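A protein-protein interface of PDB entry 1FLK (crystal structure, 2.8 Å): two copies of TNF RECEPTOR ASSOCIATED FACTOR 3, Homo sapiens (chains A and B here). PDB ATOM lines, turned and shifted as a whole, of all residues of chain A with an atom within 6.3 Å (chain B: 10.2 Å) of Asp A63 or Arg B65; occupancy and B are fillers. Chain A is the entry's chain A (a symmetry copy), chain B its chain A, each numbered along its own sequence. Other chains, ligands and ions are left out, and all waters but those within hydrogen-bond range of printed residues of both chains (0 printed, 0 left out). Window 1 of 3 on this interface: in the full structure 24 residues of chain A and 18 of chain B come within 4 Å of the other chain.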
ATOM      1  N   ARG A  58     -19.371 -27.063  12.167  1.00  0.00           N
ATOM      2  CA  ARG A  58     -19.220 -26.074  13.234  1.00  0.00           C
ATOM      3  C   ARG A  58     -19.448 -24.687  12.627  1.00  0.00           C
ATOM      4  O   ARG A  58     -20.310 -23.940  13.093  1.00  0.00           O
ATOM      5  CB  ARG A  58     -17.810 -26.130  13.844  1.00  0.00           C
ATOM      6  CG  ARG A  58     -17.273 -27.535  14.132  1.00  0.00           C
ATOM      7  CD  ARG A  58     -17.110 -27.851  15.629  1.00  0.00           C
ATOM      8  NE  ARG A  58     -16.060 -27.082  16.302  1.00  0.00           N
ATOM      9  CZ  ARG A  58     -16.280 -26.002  17.047  1.00  0.00           C
ATOM     10  NH1 ARG A  58     -17.519 -25.550  17.220  1.00  0.00           N
ATOM     11  NH2 ARG A  58     -15.262 -25.373  17.632  1.00  0.00           N
ATOM     12  N   LEU A  59     -18.672 -24.358  11.585  1.00  0.00           N
ATOM     13  CA  LEU A  59     -18.787 -23.067  10.892  1.00  0.00           C
ATOM     14  C   LEU A  59     -20.229 -22.775  10.552  1.00  0.00           C
ATOM     15  O   LEU A  59     -20.700 -21.657  10.743  1.00  0.00           O
ATOM     16  CB  LEU A  59     -17.957 -23.055   9.606  1.00  0.00           C
ATOM     17  CG  LEU A  59     -16.442 -22.857   9.748  1.00  0.00           C
ATOM     18  CD1 LEU A  59     -15.774 -22.947   8.403  1.00  0.00           C
ATOM     19  CD2 LEU A  59     -16.164 -21.499  10.368  1.00  0.00           C
ATOM     20  N   ALA A  60     -20.930 -23.795  10.065  1.00  0.00           N
ATOM     21  CA  ALA A  60     -22.338 -23.685   9.690  1.00  0.00           C
ATOM     22  C   ALA A  60     -23.272 -23.220  10.821  1.00  0.00           C
ATOM     23  O   ALA A  60     -24.206 -22.450  10.589  1.00  0.00           O
ATOM     24  CB  ALA A  60     -22.818 -25.023   9.140  1.00  0.00           C
ATOM     25  N   ASP A  61     -23.028 -23.683  12.043  1.00  0.00           N
ATOM     26  CA  ASP A  61     -23.880 -23.290  13.162  1.00  0.00           C
ATOM     27  C   ASP A  61     -23.644 -21.848  13.601  1.00  0.00           C
ATOM     28  O   ASP A  61     -24.480 -21.261  14.290  1.00  0.00           O
ATOM     29  CB  ASP A  61     -23.674 -24.231  14.352  1.00  0.00           C
ATOM     30  CG  ASP A  61     -23.805 -25.694  13.967  1.00  0.00           C
ATOM     31  OD1 ASP A  61     -22.867 -26.237  13.345  1.00  0.00           O
ATOM     32  OD2 ASP A  61     -24.853 -26.301  14.275  1.00  0.00           O
ATOM     33  N   MET A  62     -22.510 -21.277  13.193  1.00  0.00           N
ATOM     34  CA  MET A  62     -22.157 -19.899  13.550  1.00  0.00           C
ATOM     35  C   MET A  62     -23.073 -18.897  12.862  1.00  0.00           C
ATOM     36  O   MET A  62     -23.531 -17.923  13.469  1.00  0.00           O
ATOM     37  CB  MET A  62     -20.714 -19.601  13.154  1.00  0.00           C
ATOM     38  CG  MET A  62     -19.854 -19.071  14.292  1.00  0.00           C
ATOM     39  SD  MET A  62     -19.396 -20.361  15.480  1.00  0.00           S
ATOM     40  CE  MET A  62     -17.974 -21.142  14.614  1.00  0.00           C
ATOM     41  N   ASP A  63     -23.326 -19.138  11.585  1.00  0.00           N
ATOM     42  CA  ASP A  63     -24.193 -18.263  10.826  1.00  0.00           C
ATOM     43  C   ASP A  63     -25.535 -18.140  11.553  1.00  0.00           C
ATOM     44  O   ASP A  63     -25.969 -17.037  11.894  1.00  0.00           O
ATOM     45  CB  ASP A  63     -24.399 -18.826   9.418  1.00  0.00           C
ATOM     46  CG  ASP A  63     -23.109 -18.910   8.620  1.00  0.00           C
ATOM     47  OD1 ASP A  63     -22.451 -17.858   8.451  1.00  0.00           O
ATOM     48  OD2 ASP A  63     -22.752 -20.016   8.155  1.00  0.00           O
ATOM     49  N   LEU A  64     -26.182 -19.278  11.794  1.00  0.00           N
ATOM     50  CA  LEU A  64     -27.467 -19.303  12.475  1.00  0.00           C
ATOM     51  C   LEU A  64     -27.373 -18.517  13.772  1.00  0.00           C
ATOM     52  O   LEU A  64     -28.190 -17.639  14.033  1.00  0.00           O
ATOM     53  CB  LEU A  64     -27.863 -20.751  12.763  1.00  0.00           C
ATOM     54  CG  LEU A  64     -29.262 -21.202  12.334  1.00  0.00           C
ATOM     55  CD1 LEU A  64     -30.307 -20.545  13.195  1.00  0.00           C
ATOM     56  CD2 LEU A  64     -29.478 -20.845  10.874  1.00  0.00           C
ATOM     57  N   ARG A  65     -26.351 -18.847  14.566  1.00  0.00           N
ATOM     58  CA  ARG A  65     -26.048 -18.223  15.867  1.00  0.00           C
ATOM     59  C   ARG A  65     -25.911 -16.696  15.727  1.00  0.00           C
ATOM     60  O   ARG A  65     -26.330 -15.947  16.613  1.00  0.00           O
ATOM     61  CB  ARG A  65     -24.759 -18.853  16.419  1.00  0.00           C
ATOM     62  CG  ARG A  65     -24.296 -18.408  17.816  1.00  0.00           C
ATOM     63  CD  ARG A  65     -24.858 -19.252  18.955  1.00  0.00           C
ATOM     64  NE  ARG A  65     -23.961 -19.308  20.114  1.00  0.00           N
ATOM     65  CZ  ARG A  65     -22.798 -19.959  20.128  1.00  0.00           C
ATOM     66  NH1 ARG A  65     -22.378 -20.615  19.040  1.00  0.00           N
ATOM     67  NH2 ARG A  65     -22.059 -19.975  21.238  1.00  0.00           N
ATOM     68  N   PHE A  66     -25.322 -16.248  14.614  1.00  0.00           N
ATOM     69  CA  PHE A  66     -25.180 -14.815  14.304  1.00  0.00           C
ATOM     70  C   PHE A  66     -26.563 -14.322  13.853  1.00  0.00           C
ATOM     71  O   PHE A  66     -27.059 -13.280  14.298  1.00  0.00           O
ATOM     72  CB  PHE A  66     -24.225 -14.609  13.124  1.00  0.00           C
ATOM     73  CG  PHE A  66     -22.842 -14.150  13.503  1.00  0.00           C
ATOM     74  CD1 PHE A  66     -21.716 -14.819  12.999  1.00  0.00           C
ATOM     75  CD2 PHE A  66     -22.657 -13.052  14.338  1.00  0.00           C
ATOM     76  CE1 PHE A  66     -20.427 -14.407  13.322  1.00  0.00           C
ATOM     77  CE2 PHE A  66     -21.365 -12.624  14.669  1.00  0.00           C
ATOM     78  CZ  PHE A  66     -20.247 -13.307  14.160  1.00  0.00           C
ATOM     79  N   GLN A  67     -27.158 -15.108  12.949  1.00  0.00           N
ATOM     80  CA  GLN A  67     -28.467 -14.853  12.342  1.00  0.00           C
ATOM     81  C   GLN A  67     -29.607 -14.654  13.329  1.00  0.00           C
ATOM     82  O   GLN A  67     -30.444 -13.769  13.149  1.00  0.00           O
ATOM     83  CB  GLN A  67     -28.807 -16.000  11.395  1.00  0.00           C
ATOM     84  CG  GLN A  67     -30.117 -15.830  10.650  1.00  0.00           C
ATOM     85  CD  GLN A  67     -30.335 -16.900   9.590  1.00  0.00           C
ATOM     86  OE1 GLN A  67     -31.410 -16.981   8.988  1.00  0.00           O
ATOM     87  NE2 GLN A  67     -29.312 -17.725   9.353  1.00  0.00           N
ATOM     88  N   VAL A  68     -29.639 -15.490  14.363  1.00  0.00           N
ATOM     89  CA  VAL A  68     -30.668 -15.409  15.399  1.00  0.00           C
ATOM     90  C   VAL A  68     -30.373 -14.197  16.289  1.00  0.00           C
ATOM     91  O   VAL A  68     -31.282 -13.557  16.825  1.00  0.00           O
ATOM     92  CB  VAL A  68     -30.682 -16.692  16.288  1.00  0.00           C
ATOM     93  CG1 VAL A  68     -31.910 -16.706  17.145  1.00  0.00           C
ATOM     94  CG2 VAL A  68     -30.640 -17.934  15.432  1.00  0.00           C
ATOM     95  N   GLU A  70     -28.518 -11.380  15.243  1.00  0.00           N
ATOM     96  CA  GLU A  70     -28.676 -10.162  14.454  1.00  0.00           C
ATOM     97  C   GLU A  70     -30.144  -9.736  14.400  1.00  0.00           C
ATOM     98  O   GLU A  70     -30.451  -8.557  14.256  1.00  0.00           O
ATOM     99  CB  GLU A  70     -28.179 -10.387  13.029  1.00  0.00           C
ATOM    100  CG  GLU A  70     -26.772 -10.904  12.935  1.00  0.00           C
ATOM    101  CD  GLU A  70     -26.403 -11.304  11.523  1.00  0.00           C
ATOM    102  OE1 GLU A  70     -27.301 -11.776  10.796  1.00  0.00           O
ATOM    103  OE2 GLU A  70     -25.221 -11.163  11.141  1.00  0.00           O
ATOM    104  N   HIS B  55     -12.381 -22.289   4.260  1.00  0.00           N
ATOM    105  CA  HIS B  55     -12.606 -22.201   5.708  1.00  0.00           C
ATOM    106  C   HIS B  55     -11.797 -21.067   6.355  1.00  0.00           C
ATOM    107  O   HIS B  55     -12.252 -20.439   7.317  1.00  0.00           O
ATOM    108  CB  HIS B  55     -12.251 -23.529   6.379  1.00  0.00           C
ATOM    109  CG  HIS B  55     -13.306 -24.588   6.240  1.00  0.00           C
ATOM    110  ND1 HIS B  55     -13.570 -25.237   5.052  1.00  0.00           N
ATOM    111  CD2 HIS B  55     -14.143 -25.133   7.156  1.00  0.00           C
ATOM    112  CE1 HIS B  55     -14.519 -26.135   5.244  1.00  0.00           C
ATOM    113  NE2 HIS B  55     -14.884 -26.092   6.511  1.00  0.00           N
ATOM    114  N   ILE B  57     -11.085 -18.270   4.898  1.00  0.00           N
ATOM    115  CA  ILE B  57     -11.800 -17.049   4.512  1.00  0.00           C
ATOM    116  C   ILE B  57     -13.105 -16.911   5.289  1.00  0.00           C
ATOM    117  O   ILE B  57     -13.445 -15.822   5.749  1.00  0.00           O
ATOM    118  CB  ILE B  57     -12.129 -17.057   3.011  1.00  0.00           C
ATOM    119  CG1 ILE B  57     -10.829 -17.042   2.205  1.00  0.00           C
ATOM    120  CG2 ILE B  57     -13.022 -15.890   2.667  1.00  0.00           C
ATOM    121  CD1 ILE B  57     -10.985 -17.446   0.765  1.00  0.00           C
ATOM    122  N   ARG B  58     -13.831 -18.023   5.422  1.00  0.00           N
ATOM    123  CA  ARG B  58     -15.093 -18.045   6.162  1.00  0.00           C
ATOM    124  C   ARG B  58     -14.825 -17.504   7.568  1.00  0.00           C
ATOM    125  O   ARG B  58     -15.465 -16.543   7.997  1.00  0.00           O
ATOM    126  CB  ARG B  58     -15.646 -19.475   6.270  1.00  0.00           C
ATOM    127  CG  ARG B  58     -15.594 -20.300   4.981  1.00  0.00           C
ATOM    128  CD  ARG B  58     -16.975 -20.623   4.386  1.00  0.00           C
ATOM    129  NE  ARG B  58     -17.785 -21.541   5.191  1.00  0.00           N
ATOM    130  CZ  ARG B  58     -18.763 -21.160   6.010  1.00  0.00           C
ATOM    131  NH1 ARG B  58     -19.059 -19.869   6.141  1.00  0.00           N
ATOM    132  NH2 ARG B  58     -19.455 -22.069   6.694  1.00  0.00           N
ATOM    133  N   LEU B  59     -13.871 -18.127   8.274  1.00  0.00           N
ATOM    134  CA  LEU B  59     -13.494 -17.710   9.632  1.00  0.00           C
ATOM    135  C   LEU B  59     -13.259 -16.218   9.682  1.00  0.00           C
ATOM    136  O   LEU B  59     -13.710 -15.547  10.607  1.00  0.00           O
ATOM    137  CB  LEU B  59     -12.228 -18.432  10.101  1.00  0.00           C
ATOM    138  CG  LEU B  59     -12.382 -19.883  10.577  1.00  0.00           C
ATOM    139  CD1 LEU B  59     -11.039 -20.464  10.927  1.00  0.00           C
ATOM    140  CD2 LEU B  59     -13.292 -19.925  11.793  1.00  0.00           C
ATOM    141  N   ALA B  60     -12.564 -15.705   8.671  1.00  0.00           N
ATOM    142  CA  ALA B  60     -12.253 -14.281   8.561  1.00  0.00           C
ATOM    143  C   ALA B  60     -13.479 -13.352   8.560  1.00  0.00           C
ATOM    144  O   ALA B  60     -13.447 -12.268   9.149  1.00  0.00           O
ATOM    145  CB  ALA B  60     -11.420 -14.043   7.308  1.00  0.00           C
ATOM    146  N   ASP B  61     -14.557 -13.764   7.902  1.00  0.00           N
ATOM    147  CA  ASP B  61     -15.753 -12.928   7.851  1.00  0.00           C
ATOM    148  C   ASP B  61     -16.506 -12.900   9.178  1.00  0.00           C
ATOM    149  O   ASP B  61     -17.327 -12.010   9.409  1.00  0.00           O
ATOM    150  CB  ASP B  61     -16.692 -13.397   6.736  1.00  0.00           C
ATOM    151  CG  ASP B  61     -15.984 -13.535   5.399  1.00  0.00           C
ATOM    152  OD1 ASP B  61     -15.237 -14.519   5.216  1.00  0.00           O
ATOM    153  OD2 ASP B  61     -16.166 -12.654   4.534  1.00  0.00           O
ATOM    154  N   MET B  62     -16.217 -13.867  10.049  1.00  0.00           N
ATOM    155  CA  MET B  62     -16.873 -13.959  11.357  1.00  0.00           C
ATOM    156  C   MET B  62     -16.452 -12.817  12.271  1.00  0.00           C
ATOM    157  O   MET B  62     -17.274 -12.215  12.969  1.00  0.00           O
ATOM    158  CB  MET B  62     -16.527 -15.284  12.032  1.00  0.00           C
ATOM    159  CG  MET B  62     -17.739 -16.094  12.467  1.00  0.00           C
ATOM    160  SD  MET B  62     -18.591 -16.880  11.073  1.00  0.00           S
ATOM    161  CE  MET B  62     -17.541 -18.368  10.818  1.00  0.00           C
ATOM    162  N   ASP B  63     -15.158 -12.533  12.270  1.00  0.00           N
ATOM    163  CA  ASP B  63     -14.637 -11.460  13.088  1.00  0.00           C
ATOM    164  C   ASP B  63     -15.400 -10.171  12.763  1.00  0.00           C
ATOM    165  O   ASP B  63     -15.993  -9.550  13.648  1.00  0.00           O
ATOM    166  CB  ASP B  63     -13.143 -11.276  12.817  1.00  0.00           C
ATOM    167  CG  ASP B  63     -12.321 -12.501  13.184  1.00  0.00           C
ATOM    168  OD1 ASP B  63     -12.385 -12.922  14.362  1.00  0.00           O
ATOM    169  OD2 ASP B  63     -11.608 -13.040  12.307  1.00  0.00           O
ATOM    170  N   LEU B  64     -15.386  -9.783  11.490  1.00  0.00           N
ATOM    171  CA  LEU B  64     -16.069  -8.577  11.046  1.00  0.00           C
ATOM    172  C   LEU B  64     -17.510  -8.599  11.530  1.00  0.00           C
ATOM    173  O   LEU B  64     -17.980  -7.642  12.137  1.00  0.00           O
ATOM    174  CB  LEU B  64     -16.025  -8.500   9.521  1.00  0.00           C
ATOM    175  CG  LEU B  64     -15.532  -7.194   8.892  1.00  0.00           C
ATOM    176  CD1 LEU B  64     -16.541  -6.098   9.108  1.00  0.00           C
ATOM    177  CD2 LEU B  64     -14.197  -6.813   9.507  1.00  0.00           C
ATOM    178  N   ARG B  65     -18.187  -9.718  11.255  1.00  0.00           N
ATOM    179  CA  ARG B  65     -19.589  -9.976  11.628  1.00  0.00           C
ATOM    180  C   ARG B  65     -19.800  -9.795  13.141  1.00  0.00           C
ATOM    181  O   ARG B  65     -20.842  -9.295  13.572  1.00  0.00           O
ATOM    182  CB  ARG B  65     -19.957 -11.399  11.176  1.00  0.00           C
ATOM    183  CG  ARG B  65     -21.409 -11.856  11.390  1.00  0.00           C
ATOM    184  CD  ARG B  65     -22.335 -11.552  10.218  1.00  0.00           C
ATOM    185  NE  ARG B  65     -23.433 -12.518  10.098  1.00  0.00           N
ATOM    186  CZ  ARG B  65     -23.274 -13.786   9.720  1.00  0.00           C
ATOM    187  NH1 ARG B  65     -22.057 -14.255   9.422  1.00  0.00           N
ATOM    188  NH2 ARG B  65     -24.337 -14.586   9.615  1.00  0.00           N
ATOM    189  N   PHE B  66     -18.808 -10.207  13.937  1.00  0.00           N
ATOM    190  CA  PHE B  66     -18.832 -10.038  15.400  1.00  0.00           C
ATOM    191  C   PHE B  66     -18.533  -8.557  15.678  1.00  0.00           C
ATOM    192  O   PHE B  66     -19.215  -7.893  16.469  1.00  0.00           O
ATOM    193  CB  PHE B  66     -17.711 -10.851  16.057  1.00  0.00           C
ATOM    194  CG  PHE B  66     -18.158 -12.136  16.701  1.00  0.00           C
ATOM    195  CD1 PHE B  66     -17.492 -13.337  16.411  1.00  0.00           C
ATOM    196  CD2 PHE B  66     -19.219 -12.154  17.603  1.00  0.00           C
ATOM    197  CE1 PHE B  66     -17.875 -14.536  17.003  1.00  0.00           C
ATOM    198  CE2 PHE B  66     -19.614 -13.353  18.208  1.00  0.00           C
ATOM    199  CZ  PHE B  66     -18.939 -14.548  17.905  1.00  0.00           C
ATOM    200  N   GLN B  67     -17.486  -8.072  15.003  1.00  0.00           N
ATOM    201  CA  GLN B  67     -16.979  -6.701  15.104  1.00  0.00           C
ATOM    202  C   GLN B  67     -18.008  -5.613  14.838  1.00  0.00           C
ATOM    203  O   GLN B  67     -18.052  -4.606  15.544  1.00  0.00           O
ATOM    204  CB  GLN B  67     -15.801  -6.535  14.148  1.00  0.00           C
ATOM    205  CG  GLN B  67     -15.141  -5.170  14.200  1.00  0.00           C
ATOM    206  CD  GLN B  67     -13.868  -5.100  13.367  1.00  0.00           C
ATOM    207  OE1 GLN B  67     -13.285  -4.026  13.197  1.00  0.00           O
ATOM    208  NE2 GLN B  67     -13.429  -6.249  12.849  1.00  0.00           N
ATOM    209  N   VAL B  68     -18.823  -5.818  13.807  1.00  0.00           N
ATOM    210  CA  VAL B  68     -19.870  -4.865  13.440  1.00  0.00           C
ATOM    211  C   VAL B  68     -21.008  -4.970  14.461  1.00  0.00           C
ATOM    212  O   VAL B  68     -21.695  -3.990  14.762  1.00  0.00           O
ATOM    213  CB  VAL B  68     -20.441  -5.168  12.020  1.00  0.00           C
ATOM    214  CG1 VAL B  68     -21.297  -4.029  11.560  1.00  0.00           C
ATOM    215  CG2 VAL B  68     -19.324  -5.400  11.034  1.00  0.00           C
ATOM    216  N   LEU B  69     -21.190  -6.172  14.999  1.00  0.00           N
ATOM    217  CA  LEU B  69     -22.239  -6.422  15.979  1.00  0.00           C
ATOM    218  C   LEU B  69     -21.849  -5.909  17.368  1.00  0.00           C
ATOM    219  O   LEU B  69     -22.665  -5.289  18.065  1.00  0.00           O
ATOM    220  CB  LEU B  69     -22.555  -7.926  16.018  1.00  0.00           C
ATOM    221  CG  LEU B  69     -23.799  -8.418  16.767  1.00  0.00           C
ATOM    222  CD1 LEU B  69     -25.015  -7.575  16.401  1.00  0.00           C
ATOM    223  CD2 LEU B  69     -24.025  -9.887  16.434  1.00  0.00           C
ATOM    224  N   GLU B  70     -20.599  -6.151  17.765  1.00  0.00           N
ATOM    225  CA  GLU B  70     -20.113  -5.699  19.066  1.00  0.00           C
ATOM    226  C   GLU B  70     -20.186  -4.176  19.175  1.00  0.00           C
ATOM    227  O   GLU B  70     -20.323  -3.631  20.264  1.00  0.00           O
ATOM    228  CB  GLU B  70     -18.664  -6.135  19.268  1.00  0.00           C
ATOM    229  CG  GLU B  70     -18.426  -7.608  19.092  1.00  0.00           C
ATOM    230  CD  GLU B  70     -16.954  -7.953  19.100  1.00  0.00           C
ATOM    231  OE1 GLU B  70     -16.156  -7.121  18.620  1.00  0.00           O
ATOM    232  OE2 GLU B  70     -16.591  -9.055  19.566  1.00  0.00           O
ATOM    233  N   THR B  71     -20.108  -3.499  18.031  1.00  0.00           N
ATOM    234  CA  THR B  71     -20.117  -2.038  17.970  1.00  0.00           C
ATOM    235  C   THR B  71     -21.398  -1.399  17.435  1.00  0.00           C
ATOM    236  O   THR B  71     -21.442  -0.180  17.270  1.00  0.00           O
ATOM    237  CB  THR B  71     -18.988  -1.560  17.090  1.00  0.00           C
ATOM    238  OG1 THR B  71     -19.361  -1.757  15.722  1.00  0.00           O
ATOM    239  CG2 THR B  71     -17.716  -2.370  17.368  1.00  0.00           C
ATOM    240  N   ALA B  72     -22.424  -2.209  17.163  1.00  0.00           N
ATOM    241  CA  ALA B  72     -23.710  -1.712  16.657  1.00  0.00           C
ATOM    242  C   ALA B  72     -24.630  -1.131  17.747  1.00  0.00           C
ATOM    243  O   ALA B  72     -24.750  -1.694  18.827  1.00  0.00           O
ATOM    244  CB  ALA B  72     -24.430  -2.823  15.920  1.00  0.00           C
ATOM    245  N   TYR B  74     -28.580   0.410  18.783  1.00  0.00           N
ATOM    246  CA  TYR B  74     -29.979   0.341  18.386  1.00  0.00           C
ATOM    247  C   TYR B  74     -30.841   1.438  18.970  1.00  0.00           C
ATOM    248  O   TYR B  74     -32.054   1.276  19.087  1.00  0.00           O
ATOM    249  CB  TYR B  74     -30.565  -1.031  18.757  1.00  0.00           C
ATOM    250  CG  TYR B  74     -29.752  -2.196  18.221  1.00  0.00           C
ATOM    251  CD1 TYR B  74     -28.663  -2.687  18.929  1.00  0.00           C
ATOM    252  CD2 TYR B  74     -29.994  -2.722  16.945  1.00  0.00           C
ATOM    253  CE1 TYR B  74     -27.825  -3.654  18.379  1.00  0.00           C
ATOM    254  CE2 TYR B  74     -29.155  -3.691  16.388  1.00  0.00           C
ATOM    255  CZ  TYR B  74     -28.068  -4.145  17.112  1.00  0.00           C
ATOM    256  OH  TYR B  74     -27.186  -5.052  16.563  1.00  0.00           O
ATOM    257  N   GLN B 103     -19.704   1.234  10.987  1.00  0.00           N
ATOM    258  CA  GLN B 103     -20.452   0.012  11.267  1.00  0.00           C
ATOM    259  C   GLN B 103     -21.922   0.398  11.136  1.00  0.00           C
ATOM    260  O   GLN B 103     -22.297   1.539  11.426  1.00  0.00           O
ATOM    261  CB  GLN B 103     -20.176  -0.487  12.700  1.00  0.00           C
ATOM    262  CG  GLN B 103     -20.937   0.263  13.809  1.00  0.00           C
ATOM    263  CD  GLN B 103     -20.202   1.485  14.353  1.00  0.00           C
ATOM    264  OE1 GLN B 103     -19.429   2.124  13.645  1.00  0.00           O
ATOM    265  NE2 GLN B 103     -20.458   1.819  15.617  1.00  0.00           N
ATOM    266  N   PRO B 104     -22.772  -0.525  10.669  1.00  0.00           N
ATOM    267  CA  PRO B 104     -24.174  -0.112  10.568  1.00  0.00           C
ATOM    268  C   PRO B 104     -24.747   0.167  11.950  1.00  0.00           C
ATOM    269  O   PRO B 104     -24.160  -0.227  12.959  1.00  0.00           O
ATOM    270  CB  PRO B 104     -24.837  -1.309   9.901  1.00  0.00           C
ATOM    271  CG  PRO B 104     -23.750  -1.825   9.012  1.00  0.00           C
ATOM    272  CD  PRO B 104     -22.527  -1.755   9.900  1.00  0.00           C
ATOM    273  N   TYR B 106     -28.838   1.478  14.048  1.00  0.00           N
ATOM    274  CA  TYR B 106     -30.277   1.654  13.883  1.00  0.00           C
ATOM    275  C   TYR B 106     -30.911   2.692  14.806  1.00  0.00           C
ATOM    276  O   TYR B 106     -30.237   3.307  15.636  1.00  0.00           O
ATOM    277  CB  TYR B 106     -30.986   0.300  14.094  1.00  0.00           C
ATOM    278  CG  TYR B 106     -30.369  -0.839  13.319  1.00  0.00           C
ATOM    279  CD1 TYR B 106     -29.086  -1.278  13.597  1.00  0.00           C
ATOM    280  CD2 TYR B 106     -31.022  -1.403  12.243  1.00  0.00           C
ATOM    281  CE1 TYR B 106     -28.461  -2.236  12.815  1.00  0.00           C
ATOM    282  CE2 TYR B 106     -30.407  -2.369  11.450  1.00  0.00           C
ATOM    283  CZ  TYR B 106     -29.125  -2.774  11.739  1.00  0.00           C
ATOM    284  OH  TYR B 106     -28.484  -3.679  10.923  1.00  0.00           O
ATOM    285  N   LYS B 113     -32.200   1.181   9.140  1.00  0.00           N
ATOM    286  CA  LYS B 113     -30.789   0.787   9.183  1.00  0.00           C
ATOM    287  C   LYS B 113     -29.998   1.932   8.566  1.00  0.00           C
ATOM    288  O   LYS B 113     -30.455   2.564   7.603  1.00  0.00           O
ATOM    289  CB  LYS B 113     -30.511  -0.461   8.355  1.00  0.00           C
ATOM    290  CG  LYS B 113     -29.041  -0.707   8.223  1.00  0.00           C
ATOM    291  CD  LYS B 113     -28.719  -1.993   7.534  1.00  0.00           C
ATOM    292  CE  LYS B 113     -27.289  -2.385   7.875  1.00  0.00           C
ATOM    293  NZ  LYS B 113     -26.798  -3.620   7.192  1.00  0.00           N
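OD1 of Asp A63 is in salt-bridge range of NH1 of Arg B65 (3.8 Å). The guanidinium group (NE) of Arg B65 is in salt-bridge range of the side-chain carboxylate (OE2) of Glu A70.
Among the printed residues, merely in contact across the chains: Leu A59 with His B55 (3.0 Å), Leu A59 with Arg B58 (3.4 Å), Leu A59 with Leu B59 (3.6 Å), Leu A59 with Met B62 (3.4 Å), Phe A66 with Met B62 (3.3 Å), Phe A66 with Arg B65 (3.3 Å) and Phe A66 with Phe B66 (3.4 Å).
No residue of chain B comes within 4 Å of Ala A60. Asp A63 touches just one residue of chain B: Arg B65. No residue of chain B comes within 4 Å of Leu A64. Phe A66 touches three residues of chain B. Of the printed residues of chain B, Glu A70 touches Arg B65 (2.5 Å). Printed residues of chain A within 4 Å of His B55: Leu A59 (3.0 Å). Of the printed residues of chain A, Arg B58 touches Leu A59 (3.4 Å). Printed residues of chain A within 4 Å of Leu B59: Leu A59. Of the printed residues of chain A, Met B62 touches Leu A59 (3.4 Å) and Phe A66 (3.3 Å). Arg B65 touches just these residues of chain A: Asp A63 (3.7 Å), Phe A66 (3.3 Å) and Glu A70 (2.5 Å). The nearest residue of chain B that does not touch Asp A63 is Arg B58 (4.1 Å). The nearest residue of chain A that does not touch Arg B65 is Gln A67 (4.4 Å). The nearest printed residue of chain A that does not touch Met B62 is Met A62 (4.03 Å).
Of the 22 printed residues of chain B, 6 touch a printed residue of chain A. Printed residues of chain B that touch a printed residue of chain A: His B55, Arg B58, Leu B59, Met B62, Arg B65 and Phe B66. Hydrophobic or aromatic side chains of chain B within 4 Å of the printed part of chain A: His B55, Leu B59, Met B62 and Phe B66. Printed residues of chain A that touch a printed residue of chain B: Leu A59, Asp A63, Phe A66 and Glu A70. Hydrophobic or aromatic side chains of chain A within 4 Å of the printed part of chain B: Leu A59 and Phe A66. Among the printed residues, Asp or Glu carboxylates within 4 Å of a Lys or Arg side-chain nitrogen of the other chain: Asp A63 with Arg B65 and Glu A70 with Arg B65.
Leu A59 touches Arg B58, but with the chains exchanged Arg A58 does not touch Leu B59 (7.8 Å). Leu A59 touches Met B62, but with the chains exchanged Met A62 does not touch Leu B59 (5.6 Å). Phe A66 touches Met B62, but with the chains exchanged Met A62 does not touch Phe B66 (5.6 Å). Phe A66 touches Arg B65, but with the chains exchanged Arg A65 does not touch Phe B66 (6.6 Å). Positions printed for both chains: 58, 59, 60, 61, 62, 63, 64, 65, 66, 67, 68 and 70.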
